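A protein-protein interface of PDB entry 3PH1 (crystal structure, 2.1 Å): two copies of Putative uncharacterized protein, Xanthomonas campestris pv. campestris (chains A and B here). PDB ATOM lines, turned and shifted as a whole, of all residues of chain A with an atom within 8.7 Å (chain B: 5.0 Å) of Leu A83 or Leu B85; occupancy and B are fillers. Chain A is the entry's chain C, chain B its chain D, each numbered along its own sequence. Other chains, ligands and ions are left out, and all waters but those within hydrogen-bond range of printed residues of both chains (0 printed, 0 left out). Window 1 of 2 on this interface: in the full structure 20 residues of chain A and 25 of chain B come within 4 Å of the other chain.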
ATOM      1  N   GLN A  75      13.976   8.798  17.337  1.00  0.00           N
ATOM      2  CA  GLN A  75      13.817   9.995  18.165  1.00  0.00           C
ATOM      3  C   GLN A  75      14.735   9.832  19.367  1.00  0.00           C
ATOM      4  O   GLN A  75      15.370  10.786  19.812  1.00  0.00           O
ATOM      5  CB  GLN A  75      12.381  10.144  18.671  1.00  0.00           C
ATOM      6  CG  GLN A  75      11.301  10.095  17.614  1.00  0.00           C
ATOM      7  CD  GLN A  75       9.916  10.368  18.192  1.00  0.00           C
ATOM      8  OE1 GLN A  75       8.904  10.065  17.563  1.00  0.00           O
ATOM      9  NE2 GLN A  75       9.868  10.953  19.394  1.00  0.00           N
ATOM     10  N   ARG A  76      14.771   8.610  19.894  1.00  0.00           N
ATOM     11  CA  ARG A  76      15.607   8.248  21.040  1.00  0.00           C
ATOM     12  C   ARG A  76      17.069   8.533  20.677  1.00  0.00           C
ATOM     13  O   ARG A  76      17.785   9.201  21.421  1.00  0.00           O
ATOM     14  CB  ARG A  76      15.403   6.757  21.365  1.00  0.00           C
ATOM     15  CG  ARG A  76      16.472   6.081  22.240  1.00  0.00           C
ATOM     16  CD  ARG A  76      16.243   4.552  22.296  1.00  0.00           C
ATOM     17  NE  ARG A  76      17.275   3.807  23.029  1.00  0.00           N
ATOM     18  CZ  ARG A  76      17.360   3.710  24.359  1.00  0.00           C
ATOM     19  NH1 ARG A  76      16.470   4.311  25.144  1.00  0.00           N
ATOM     20  NH2 ARG A  76      18.348   3.007  24.909  1.00  0.00           N
ATOM     21  N   MET A  77      17.491   8.035  19.516  1.00  0.00           N
ATOM     22  CA  MET A  77      18.850   8.239  19.038  1.00  0.00           C
ATOM     23  C   MET A  77      19.165   9.738  18.924  1.00  0.00           C
ATOM     24  O   MET A  77      20.213  10.187  19.391  1.00  0.00           O
ATOM     25  CB  MET A  77      19.043   7.515  17.697  1.00  0.00           C
ATOM     26  CG  MET A  77      19.082   5.987  17.849  1.00  0.00           C
ATOM     27  SD  MET A  77      19.004   5.026  16.317  1.00  0.00           S
ATOM     28  CE  MET A  77      20.511   5.477  15.570  1.00  0.00           C
ATOM     29  N   ASP A  78      18.258  10.507  18.328  1.00  0.00           N
ATOM     30  CA  ASP A  78      18.447  11.966  18.191  1.00  0.00           C
ATOM     31  C   ASP A  78      18.603  12.641  19.567  1.00  0.00           C
ATOM     32  O   ASP A  78      19.388  13.588  19.724  1.00  0.00           O
ATOM     33  CB  ASP A  78      17.258  12.598  17.454  1.00  0.00           C
ATOM     34  CG  ASP A  78      17.539  14.026  16.986  1.00  0.00           C
ATOM     35  OD1 ASP A  78      16.612  14.861  17.044  1.00  0.00           O
ATOM     36  OD2 ASP A  78      18.672  14.314  16.542  1.00  0.00           O
ATOM     37  N   ALA A  79      17.850  12.156  20.557  1.00  0.00           N
ATOM     38  CA  ALA A  79      17.919  12.693  21.910  1.00  0.00           C
ATOM     39  C   ALA A  79      19.324  12.467  22.474  1.00  0.00           C
ATOM     40  O   ALA A  79      19.955  13.391  23.014  1.00  0.00           O
ATOM     41  CB  ALA A  79      16.879  12.011  22.802  1.00  0.00           C
ATOM     42  N   LYS A  80      19.804  11.235  22.333  1.00  0.00           N
ATOM     43  CA  LYS A  80      21.127  10.854  22.802  1.00  0.00           C
ATOM     44  C   LYS A  80      22.215  11.709  22.156  1.00  0.00           C
ATOM     45  O   LYS A  80      23.192  12.061  22.811  1.00  0.00           O
ATOM     46  CB  LYS A  80      21.378   9.376  22.516  1.00  0.00           C
ATOM     47  CG  LYS A  80      20.375   8.445  23.198  1.00  0.00           C
ATOM     48  CD  LYS A  80      20.636   6.972  22.898  1.00  0.00           C
ATOM     49  CE  LYS A  80      19.518   6.121  23.489  1.00  0.00           C
ATOM     50  NZ  LYS A  80      19.818   4.668  23.463  1.00  0.00           N
ATOM     51  N   LEU A  81      22.047  12.043  20.879  1.00  0.00           N
ATOM     52  CA  LEU A  81      23.033  12.871  20.194  1.00  0.00           C
ATOM     53  C   LEU A  81      23.070  14.268  20.815  1.00  0.00           C
ATOM     54  O   LEU A  81      24.147  14.803  21.059  1.00  0.00           O
ATOM     55  CB  LEU A  81      22.734  12.955  18.683  1.00  0.00           C
ATOM     56  CG  LEU A  81      23.135  11.734  17.839  1.00  0.00           C
ATOM     57  CD1 LEU A  81      22.607  11.920  16.405  1.00  0.00           C
ATOM     58  CD2 LEU A  81      24.641  11.557  17.840  1.00  0.00           C
ATOM     59  N   ASP A  82      21.889  14.834  21.080  1.00  0.00           N
ATOM     60  CA  ASP A  82      21.768  16.152  21.699  1.00  0.00           C
ATOM     61  C   ASP A  82      22.499  16.139  23.036  1.00  0.00           C
ATOM     62  O   ASP A  82      23.215  17.078  23.364  1.00  0.00           O
ATOM     63  CB  ASP A  82      20.294  16.524  21.945  1.00  0.00           C
ATOM     64  CG  ASP A  82      19.549  16.892  20.665  1.00  0.00           C
ATOM     65  OD1 ASP A  82      20.192  17.484  19.774  1.00  0.00           O
ATOM     66  OD2 ASP A  82      18.331  16.612  20.558  1.00  0.00           O
ATOM     67  N   LEU A  83      22.299  15.068  23.801  1.00  0.00           N
ATOM     68  CA  LEU A  83      22.940  14.890  25.106  1.00  0.00           C
ATOM     69  C   LEU A  83      24.463  14.768  24.975  1.00  0.00           C
ATOM     70  O   LEU A  83      25.209  15.457  25.668  1.00  0.00           O
ATOM     71  CB  LEU A  83      22.372  13.642  25.803  1.00  0.00           C
ATOM     72  CG  LEU A  83      21.316  13.792  26.907  1.00  0.00           C
ATOM     73  CD1 LEU A  83      20.786  15.223  26.999  1.00  0.00           C
ATOM     74  CD2 LEU A  83      20.194  12.802  26.654  1.00  0.00           C
ATOM     75  N   ILE A  84      24.922  13.886  24.090  1.00  0.00           N
ATOM     76  CA  ILE A  84      26.354  13.714  23.895  1.00  0.00           C
ATOM     77  C   ILE A  84      26.990  15.057  23.510  1.00  0.00           C
ATOM     78  O   ILE A  84      28.007  15.460  24.078  1.00  0.00           O
ATOM     79  CB  ILE A  84      26.633  12.683  22.786  1.00  0.00           C
ATOM     80  CG1 ILE A  84      26.193  11.283  23.252  1.00  0.00           C
ATOM     81  CG2 ILE A  84      28.108  12.743  22.391  1.00  0.00           C
ATOM     82  CD1 ILE A  84      25.973  10.271  22.114  1.00  0.00           C
ATOM     83  N   LEU A  85      26.373  15.745  22.554  1.00  0.00           N
ATOM     84  CA  LEU A  85      26.869  17.031  22.073  1.00  0.00           C
ATOM     85  C   LEU A  85      26.998  18.031  23.220  1.00  0.00           C
ATOM     86  O   LEU A  85      28.009  18.704  23.358  1.00  0.00           O
ATOM     87  CB  LEU A  85      25.919  17.601  21.015  1.00  0.00           C
ATOM     88  CG  LEU A  85      26.461  18.420  19.835  1.00  0.00           C
ATOM     89  CD1 LEU A  85      25.566  19.619  19.669  1.00  0.00           C
ATOM     90  CD2 LEU A  85      27.916  18.850  20.038  1.00  0.00           C
ATOM     91  N   ALA A  86      25.963  18.124  24.041  1.00  0.00           N
ATOM     92  CA  ALA A  86      25.991  19.033  25.171  1.00  0.00           C
ATOM     93  C   ALA A  86      27.097  18.637  26.156  1.00  0.00           C
ATOM     94  O   ALA A  86      27.804  19.500  26.672  1.00  0.00           O
ATOM     95  CB  ALA A  86      24.629  19.043  25.877  1.00  0.00           C
ATOM     96  N   LEU A  87      27.246  17.340  26.416  1.00  0.00           N
ATOM     97  CA  LEU A  87      28.275  16.880  27.342  1.00  0.00           C
ATOM     98  C   LEU A  87      29.685  17.102  26.791  1.00  0.00           C
ATOM     99  O   LEU A  87      30.605  17.443  27.544  1.00  0.00           O
ATOM    100  CB  LEU A  87      28.064  15.407  27.709  1.00  0.00           C
ATOM    101  CG  LEU A  87      26.949  15.151  28.745  1.00  0.00           C
ATOM    102  CD1 LEU A  87      26.650  13.667  28.834  1.00  0.00           C
ATOM    103  CD2 LEU A  87      27.361  15.705  30.116  1.00  0.00           C
ATOM    104  N   ILE A  88      29.863  16.928  25.484  1.00  0.00           N
ATOM    105  CA  ILE A  88      31.187  17.148  24.910  1.00  0.00           C
ATOM    106  C   ILE A  88      31.502  18.644  24.986  1.00  0.00           C
ATOM    107  O   ILE A  88      32.639  19.028  25.226  1.00  0.00           O
ATOM    108  CB  ILE A  88      31.284  16.637  23.436  1.00  0.00           C
ATOM    109  CG1 ILE A  88      32.698  16.856  22.889  1.00  0.00           C
ATOM    110  CG2 ILE A  88      30.301  17.359  22.559  1.00  0.00           C
ATOM    111  CD1 ILE A  88      33.760  15.977  23.510  1.00  0.00           C
ATOM    112  N   GLY A  89      30.483  19.481  24.807  1.00  0.00           N
ATOM    113  CA  GLY A  89      30.682  20.919  24.889  1.00  0.00           C
ATOM    114  C   GLY A  89      31.047  21.316  26.309  1.00  0.00           C
ATOM    115  O   GLY A  89      31.842  22.237  26.540  1.00  0.00           O
ATOM    116  N   ARG A  90      30.456  20.616  27.273  1.00  0.00           N
ATOM    117  CA  ARG A  90      30.735  20.879  28.673  1.00  0.00           C
ATOM    118  C   ARG A  90      32.186  20.500  28.960  1.00  0.00           C
ATOM    119  O   ARG A  90      32.907  21.237  29.623  1.00  0.00           O
ATOM    120  CB  ARG A  90      29.792  20.064  29.569  1.00  0.00           C
ATOM    121  CG  ARG A  90      30.020  20.291  31.062  1.00  0.00           C
ATOM    122  CD  ARG A  90      28.892  19.718  31.898  1.00  0.00           C
ATOM    123  NE  ARG A  90      27.594  20.244  31.469  1.00  0.00           N
ATOM    124  CZ  ARG A  90      27.116  21.446  31.784  1.00  0.00           C
ATOM    125  NH1 ARG A  90      25.930  21.824  31.336  1.00  0.00           N
ATOM    126  NH2 ARG A  90      27.807  22.258  32.565  1.00  0.00           N
ATOM    127  N   LEU B  48      17.833  20.057  26.407  1.00  0.00           N
ATOM    128  CA  LEU B  48      18.215  19.186  27.508  1.00  0.00           C
ATOM    129  C   LEU B  48      17.007  18.463  28.121  1.00  0.00           C
ATOM    130  O   LEU B  48      16.991  17.237  28.246  1.00  0.00           O
ATOM    131  CB  LEU B  48      18.930  19.999  28.591  1.00  0.00           C
ATOM    132  CG  LEU B  48      19.320  19.242  29.861  1.00  0.00           C
ATOM    133  CD1 LEU B  48      20.254  18.101  29.491  1.00  0.00           C
ATOM    134  CD2 LEU B  48      19.984  20.194  30.864  1.00  0.00           C
ATOM    135  N   SER B  51      15.210  15.982  25.586  1.00  0.00           N
ATOM    136  CA  SER B  51      16.074  14.847  25.275  1.00  0.00           C
ATOM    137  C   SER B  51      16.149  13.923  26.472  1.00  0.00           C
ATOM    138  O   SER B  51      16.099  12.692  26.345  1.00  0.00           O
ATOM    139  CB  SER B  51      17.473  15.331  24.919  1.00  0.00           C
ATOM    140  OG  SER B  51      17.414  16.165  23.784  1.00  0.00           O
ATOM    141  N   LEU B  52      16.281  14.530  27.641  1.00  0.00           N
ATOM    142  CA  LEU B  52      16.353  13.774  28.872  1.00  0.00           C
ATOM    143  C   LEU B  52      15.095  12.917  28.980  1.00  0.00           C
ATOM    144  O   LEU B  52      15.174  11.711  29.193  1.00  0.00           O
ATOM    145  CB  LEU B  52      16.450  14.740  30.053  1.00  0.00           C
ATOM    146  CG  LEU B  52      17.502  14.431  31.116  1.00  0.00           C
ATOM    147  CD1 LEU B  52      18.789  13.915  30.465  1.00  0.00           C
ATOM    148  CD2 LEU B  52      17.771  15.701  31.912  1.00  0.00           C
ATOM    149  N   VAL B  55      15.159   9.716  26.831  1.00  0.00           N
ATOM    150  CA  VAL B  55      15.987   8.584  27.239  1.00  0.00           C
ATOM    151  C   VAL B  55      15.618   8.037  28.620  1.00  0.00           C
ATOM    152  O   VAL B  55      15.933   6.893  28.944  1.00  0.00           O
ATOM    153  CB  VAL B  55      17.501   8.937  27.222  1.00  0.00           C
ATOM    154  CG1 VAL B  55      17.854   9.663  25.927  1.00  0.00           C
ATOM    155  CG2 VAL B  55      17.867   9.769  28.435  1.00  0.00           C
ATOM    156  N   LYS B  80      25.929   1.914  20.151  1.00  0.00           N
ATOM    157  CA  LYS B  80      27.122   2.741  20.113  1.00  0.00           C
ATOM    158  C   LYS B  80      26.868   4.082  20.795  1.00  0.00           C
ATOM    159  O   LYS B  80      27.742   4.596  21.497  1.00  0.00           O
ATOM    160  CB  LYS B  80      27.558   2.953  18.662  1.00  0.00           C
ATOM    161  CG  LYS B  80      27.997   1.661  17.984  1.00  0.00           C
ATOM    162  CD  LYS B  80      28.443   1.881  16.565  1.00  0.00           C
ATOM    163  CE  LYS B  80      28.806   0.535  15.946  1.00  0.00           C
ATOM    164  NZ  LYS B  80      29.119   0.596  14.493  1.00  0.00           N
ATOM    165  N   LEU B  81      25.673   4.638  20.584  1.00  0.00           N
ATOM    166  CA  LEU B  81      25.298   5.915  21.199  1.00  0.00           C
ATOM    167  C   LEU B  81      25.232   5.752  22.723  1.00  0.00           C
ATOM    168  O   LEU B  81      25.680   6.629  23.463  1.00  0.00           O
ATOM    169  CB  LEU B  81      23.956   6.419  20.637  1.00  0.00           C
ATOM    170  CG  LEU B  81      23.935   7.002  19.204  1.00  0.00           C
ATOM    171  CD1 LEU B  81      22.504   7.239  18.747  1.00  0.00           C
ATOM    172  CD2 LEU B  81      24.722   8.309  19.152  1.00  0.00           C
ATOM    173  N   ASP B  82      24.697   4.622  23.190  1.00  0.00           N
ATOM    174  CA  ASP B  82      24.628   4.371  24.625  1.00  0.00           C
ATOM    175  C   ASP B  82      26.029   4.320  25.221  1.00  0.00           C
ATOM    176  O   ASP B  82      26.270   4.846  26.297  1.00  0.00           O
ATOM    177  CB  ASP B  82      23.916   3.047  24.936  1.00  0.00           C
ATOM    178  CG  ASP B  82      22.419   3.101  24.659  1.00  0.00           C
ATOM    179  OD1 ASP B  82      21.832   4.204  24.749  1.00  0.00           O
ATOM    180  OD2 ASP B  82      21.826   2.031  24.369  1.00  0.00           O
ATOM    181  N   LEU B  83      26.952   3.673  24.522  1.00  0.00           N
ATOM    182  CA  LEU B  83      28.311   3.558  25.012  1.00  0.00           C
ATOM    183  C   LEU B  83      29.000   4.909  25.021  1.00  0.00           C
ATOM    184  O   LEU B  83      29.675   5.252  25.983  1.00  0.00           O
ATOM    185  CB  LEU B  83      29.106   2.559  24.159  1.00  0.00           C
ATOM    186  CG  LEU B  83      28.662   1.090  24.243  1.00  0.00           C
ATOM    187  CD1 LEU B  83      29.487   0.229  23.286  1.00  0.00           C
ATOM    188  CD2 LEU B  83      28.822   0.594  25.682  1.00  0.00           C
ATOM    189  N   ILE B  84      28.825   5.674  23.948  1.00  0.00           N
ATOM    190  CA  ILE B  84      29.444   6.990  23.843  1.00  0.00           C
ATOM    191  C   ILE B  84      28.941   7.898  24.966  1.00  0.00           C
ATOM    192  O   ILE B  84      29.730   8.511  25.689  1.00  0.00           O
ATOM    193  CB  ILE B  84      29.121   7.655  22.473  1.00  0.00           C
ATOM    194  CG1 ILE B  84      29.838   6.908  21.344  1.00  0.00           C
ATOM    195  CG2 ILE B  84      29.497   9.140  22.511  1.00  0.00           C
ATOM    196  CD1 ILE B  84      29.358   7.280  19.937  1.00  0.00           C
ATOM    197  N   LEU B  85      27.622   7.961  25.110  1.00  0.00           N
ATOM    198  CA  LEU B  85      26.984   8.784  26.134  1.00  0.00           C
ATOM    199  C   LEU B  85      27.525   8.449  27.528  1.00  0.00           C
ATOM    200  O   LEU B  85      27.848   9.342  28.311  1.00  0.00           O
ATOM    201  CB  LEU B  85      25.467   8.567  26.082  1.00  0.00           C
ATOM    202  CG  LEU B  85      24.544   9.339  27.028  1.00  0.00           C
ATOM    203  CD1 LEU B  85      24.704  10.833  26.851  1.00  0.00           C
ATOM    204  CD2 LEU B  85      23.110   8.920  26.741  1.00  0.00           C
ATOM    205  N   ALA B  86      27.633   7.160  27.827  1.00  0.00           N
ATOM    206  CA  ALA B  86      28.136   6.717  29.126  1.00  0.00           C
ATOM    207  C   ALA B  86      29.563   7.189  29.390  1.00  0.00           C
ATOM    208  O   ALA B  86      29.862   7.709  30.468  1.00  0.00           O
ATOM    209  CB  ALA B  86      28.064   5.187  29.229  1.00  0.00           C
ATOM    210  N   LEU B  87      30.437   7.005  28.406  1.00  0.00           N
ATOM    211  CA  LEU B  87      31.831   7.416  28.538  1.00  0.00           C
ATOM    212  C   LEU B  87      31.968   8.928  28.653  1.00  0.00           C
ATOM    213  O   LEU B  87      32.685   9.417  29.523  1.00  0.00           O
ATOM    214  CB  LEU B  87      32.666   6.916  27.347  1.00  0.00           C
ATOM    215  CG  LEU B  87      33.111   5.447  27.358  1.00  0.00           C
ATOM    216  CD1 LEU B  87      34.047   5.185  26.191  1.00  0.00           C
ATOM    217  CD2 LEU B  87      33.822   5.131  28.671  1.00  0.00           C
ATOM    218  N   ILE B  88      31.273   9.666  27.787  1.00  0.00           N
ATOM    219  CA  ILE B  88      31.358  11.123  27.825  1.00  0.00           C
ATOM    220  C   ILE B  88      30.889  11.611  29.191  1.00  0.00           C
ATOM    221  O   ILE B  88      31.435  12.568  29.734  1.00  0.00           O
ATOM    222  CB  ILE B  88      30.529  11.790  26.672  1.00  0.00           C
ATOM    223  CG1 ILE B  88      30.829  13.292  26.606  1.00  0.00           C
ATOM    224  CG2 ILE B  88      29.039  11.584  26.872  1.00  0.00           C
ATOM    225  CD1 ILE B  88      32.203  13.634  26.063  1.00  0.00           C
ATOM    226  N   GLY B  89      29.893  10.926  29.756  1.00  0.00           N
ATOM    227  CA  GLY B  89      29.384  11.295  31.065  1.00  0.00           C
ATOM    228  C   GLY B  89      30.484  11.200  32.107  1.00  0.00           C
ATOM    229  O   GLY B  89      30.693  12.119  32.894  1.00  0.00           O
ATOM    230  N   TRP B 134      22.165  10.271  36.792  1.00  0.00           N
ATOM    231  CA  TRP B 134      23.117   9.474  36.006  1.00  0.00           C
ATOM    232  C   TRP B 134      23.905  10.239  34.928  1.00  0.00           C
ATOM    233  O   TRP B 134      24.833   9.684  34.342  1.00  0.00           O
ATOM    234  CB  TRP B 134      22.403   8.275  35.357  1.00  0.00           C
ATOM    235  CG  TRP B 134      21.274   8.672  34.460  1.00  0.00           C
ATOM    236  CD1 TRP B 134      20.068   9.204  34.835  1.00  0.00           C
ATOM    237  CD2 TRP B 134      21.267   8.630  33.032  1.00  0.00           C
ATOM    238  NE1 TRP B 134      19.317   9.499  33.724  1.00  0.00           N
ATOM    239  CE2 TRP B 134      20.029   9.159  32.604  1.00  0.00           C
ATOM    240  CE3 TRP B 134      22.190   8.196  32.070  1.00  0.00           C
ATOM    241  CZ2 TRP B 134      19.689   9.270  31.254  1.00  0.00           C
ATOM    242  CZ3 TRP B 134      21.852   8.303  30.723  1.00  0.00           C
ATOM    243  CH2 TRP B 134      20.610   8.838  30.329  1.00  0.00           C
ATOM    244  N   LEU B 135      23.538  11.497  34.674  1.00  0.00           N
ATOM    245  CA  LEU B 135      24.223  12.334  33.675  1.00  0.00           C
ATOM    246  C   LEU B 135      24.635  13.667  34.292  1.00  0.00           C
ATOM    247  O   LEU B 135      23.824  14.337  34.934  1.00  0.00           O
ATOM    248  CB  LEU B 135      23.304  12.613  32.488  1.00  0.00           C
ATOM    249  CG  LEU B 135      23.805  12.215  31.106  1.00  0.00           C
ATOM    250  CD1 LEU B 135      23.955  10.713  31.065  1.00  0.00           C
ATOM    251  CD2 LEU B 135      22.834  12.678  30.031  1.00  0.00           C
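Among the printed residues, pairs that only touch across the chains: Leu A81 with Leu B81, Met A77 with Leu B81, Leu A83 with Leu B135, Leu A87 with Ile B88, Ala A79 with Ser B51, Ile A84 with Ile B84, Ile A84 with Leu B81, Leu A83 with Leu B85, Ile A88 with Ile B88, Leu A83 with Leu B48, Ile A84 with Leu B85, Lys A80 with Val B55, Leu A83 with Ser B51, Leu A87 with Leu B135, Leu A87 with Leu B85 and Leu A83 with Val B55.
The side-chain carboxylate of Asp B82 lies within salt-bridge range of the guanidinium group of Arg A76, 3.7 Å away. OD2 of Asp A82 sits at hydrogen-bond distance from OG of Ser B51 (3.4 Å). The side-chain amino group (NZ) of Lys A80 lies within salt-bridge range of the side-chain carboxylate (OD1) of Asp B82 (2.4 Å).
NZ of Lys A80 lies close to NH2 of Arg A76, 2.6 Å away.
Leu A81 touches its own counterpart, Leu B81. Ile A84 touches Leu B85, but with the chains exchanged Leu A85 does not touch Ile B84 (7.3 Å). Leu A87 touches Ile B88, but with the chains exchanged Ile A88 does not touch Leu B87 (8.9 Å). Ile A88 touches its own counterpart, Ile B88.
Of the 16 printed residues of chain A, 10 touch a printed residue of chain B. Printed residues of chain A that touch a printed residue of chain B: Arg A76, Met A77, Ala A79, Lys A80, Leu A81, Asp A82, Leu A83, Ile A84, Leu A87 and Ile A88. Hydrophobic or aromatic side chains of chain A within 4 Å of the printed part of chain B: Met A77, Ala A79, Leu A81, Leu A83, Ile A84, Leu A87 and Ile A88. Among the printed residues, 19 pairs touch across the chains.
Of the printed residues of chain B, Ala A79 touches Ser B51. Of the printed residues of chain B, Leu A81 touches Leu B81. Of the printed residues of chain B, Leu A83 touches Leu B48, Ser B51, Val B55, Leu B85 and Leu B135. Printed residues of chain A within 4 Å of Leu B48: Leu A83 (3.8 Å). Of the printed residues of chain A, Leu B81 touches Met A77 (3.6 Å), Leu A81 (3.5 Å) and Ile A84 (3.8 Å). Leu B83 touches none of the printed residues of chain A. Leu B85 touches three residues of chain A. No residue of chain A comes within 4 Å of Ala B86. Gly B89 touches none of the printed residues of chain A. The nearest printed residue of chain B that does not touch Leu A83 is Leu B52 (4.2 Å). The nearest residue of chain A that does not touch Leu B85 is Lys A80 (4.5 Å). The nearest printed residue of chain B that does not touch Asp A82 is Leu B48 (6.2 Å).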
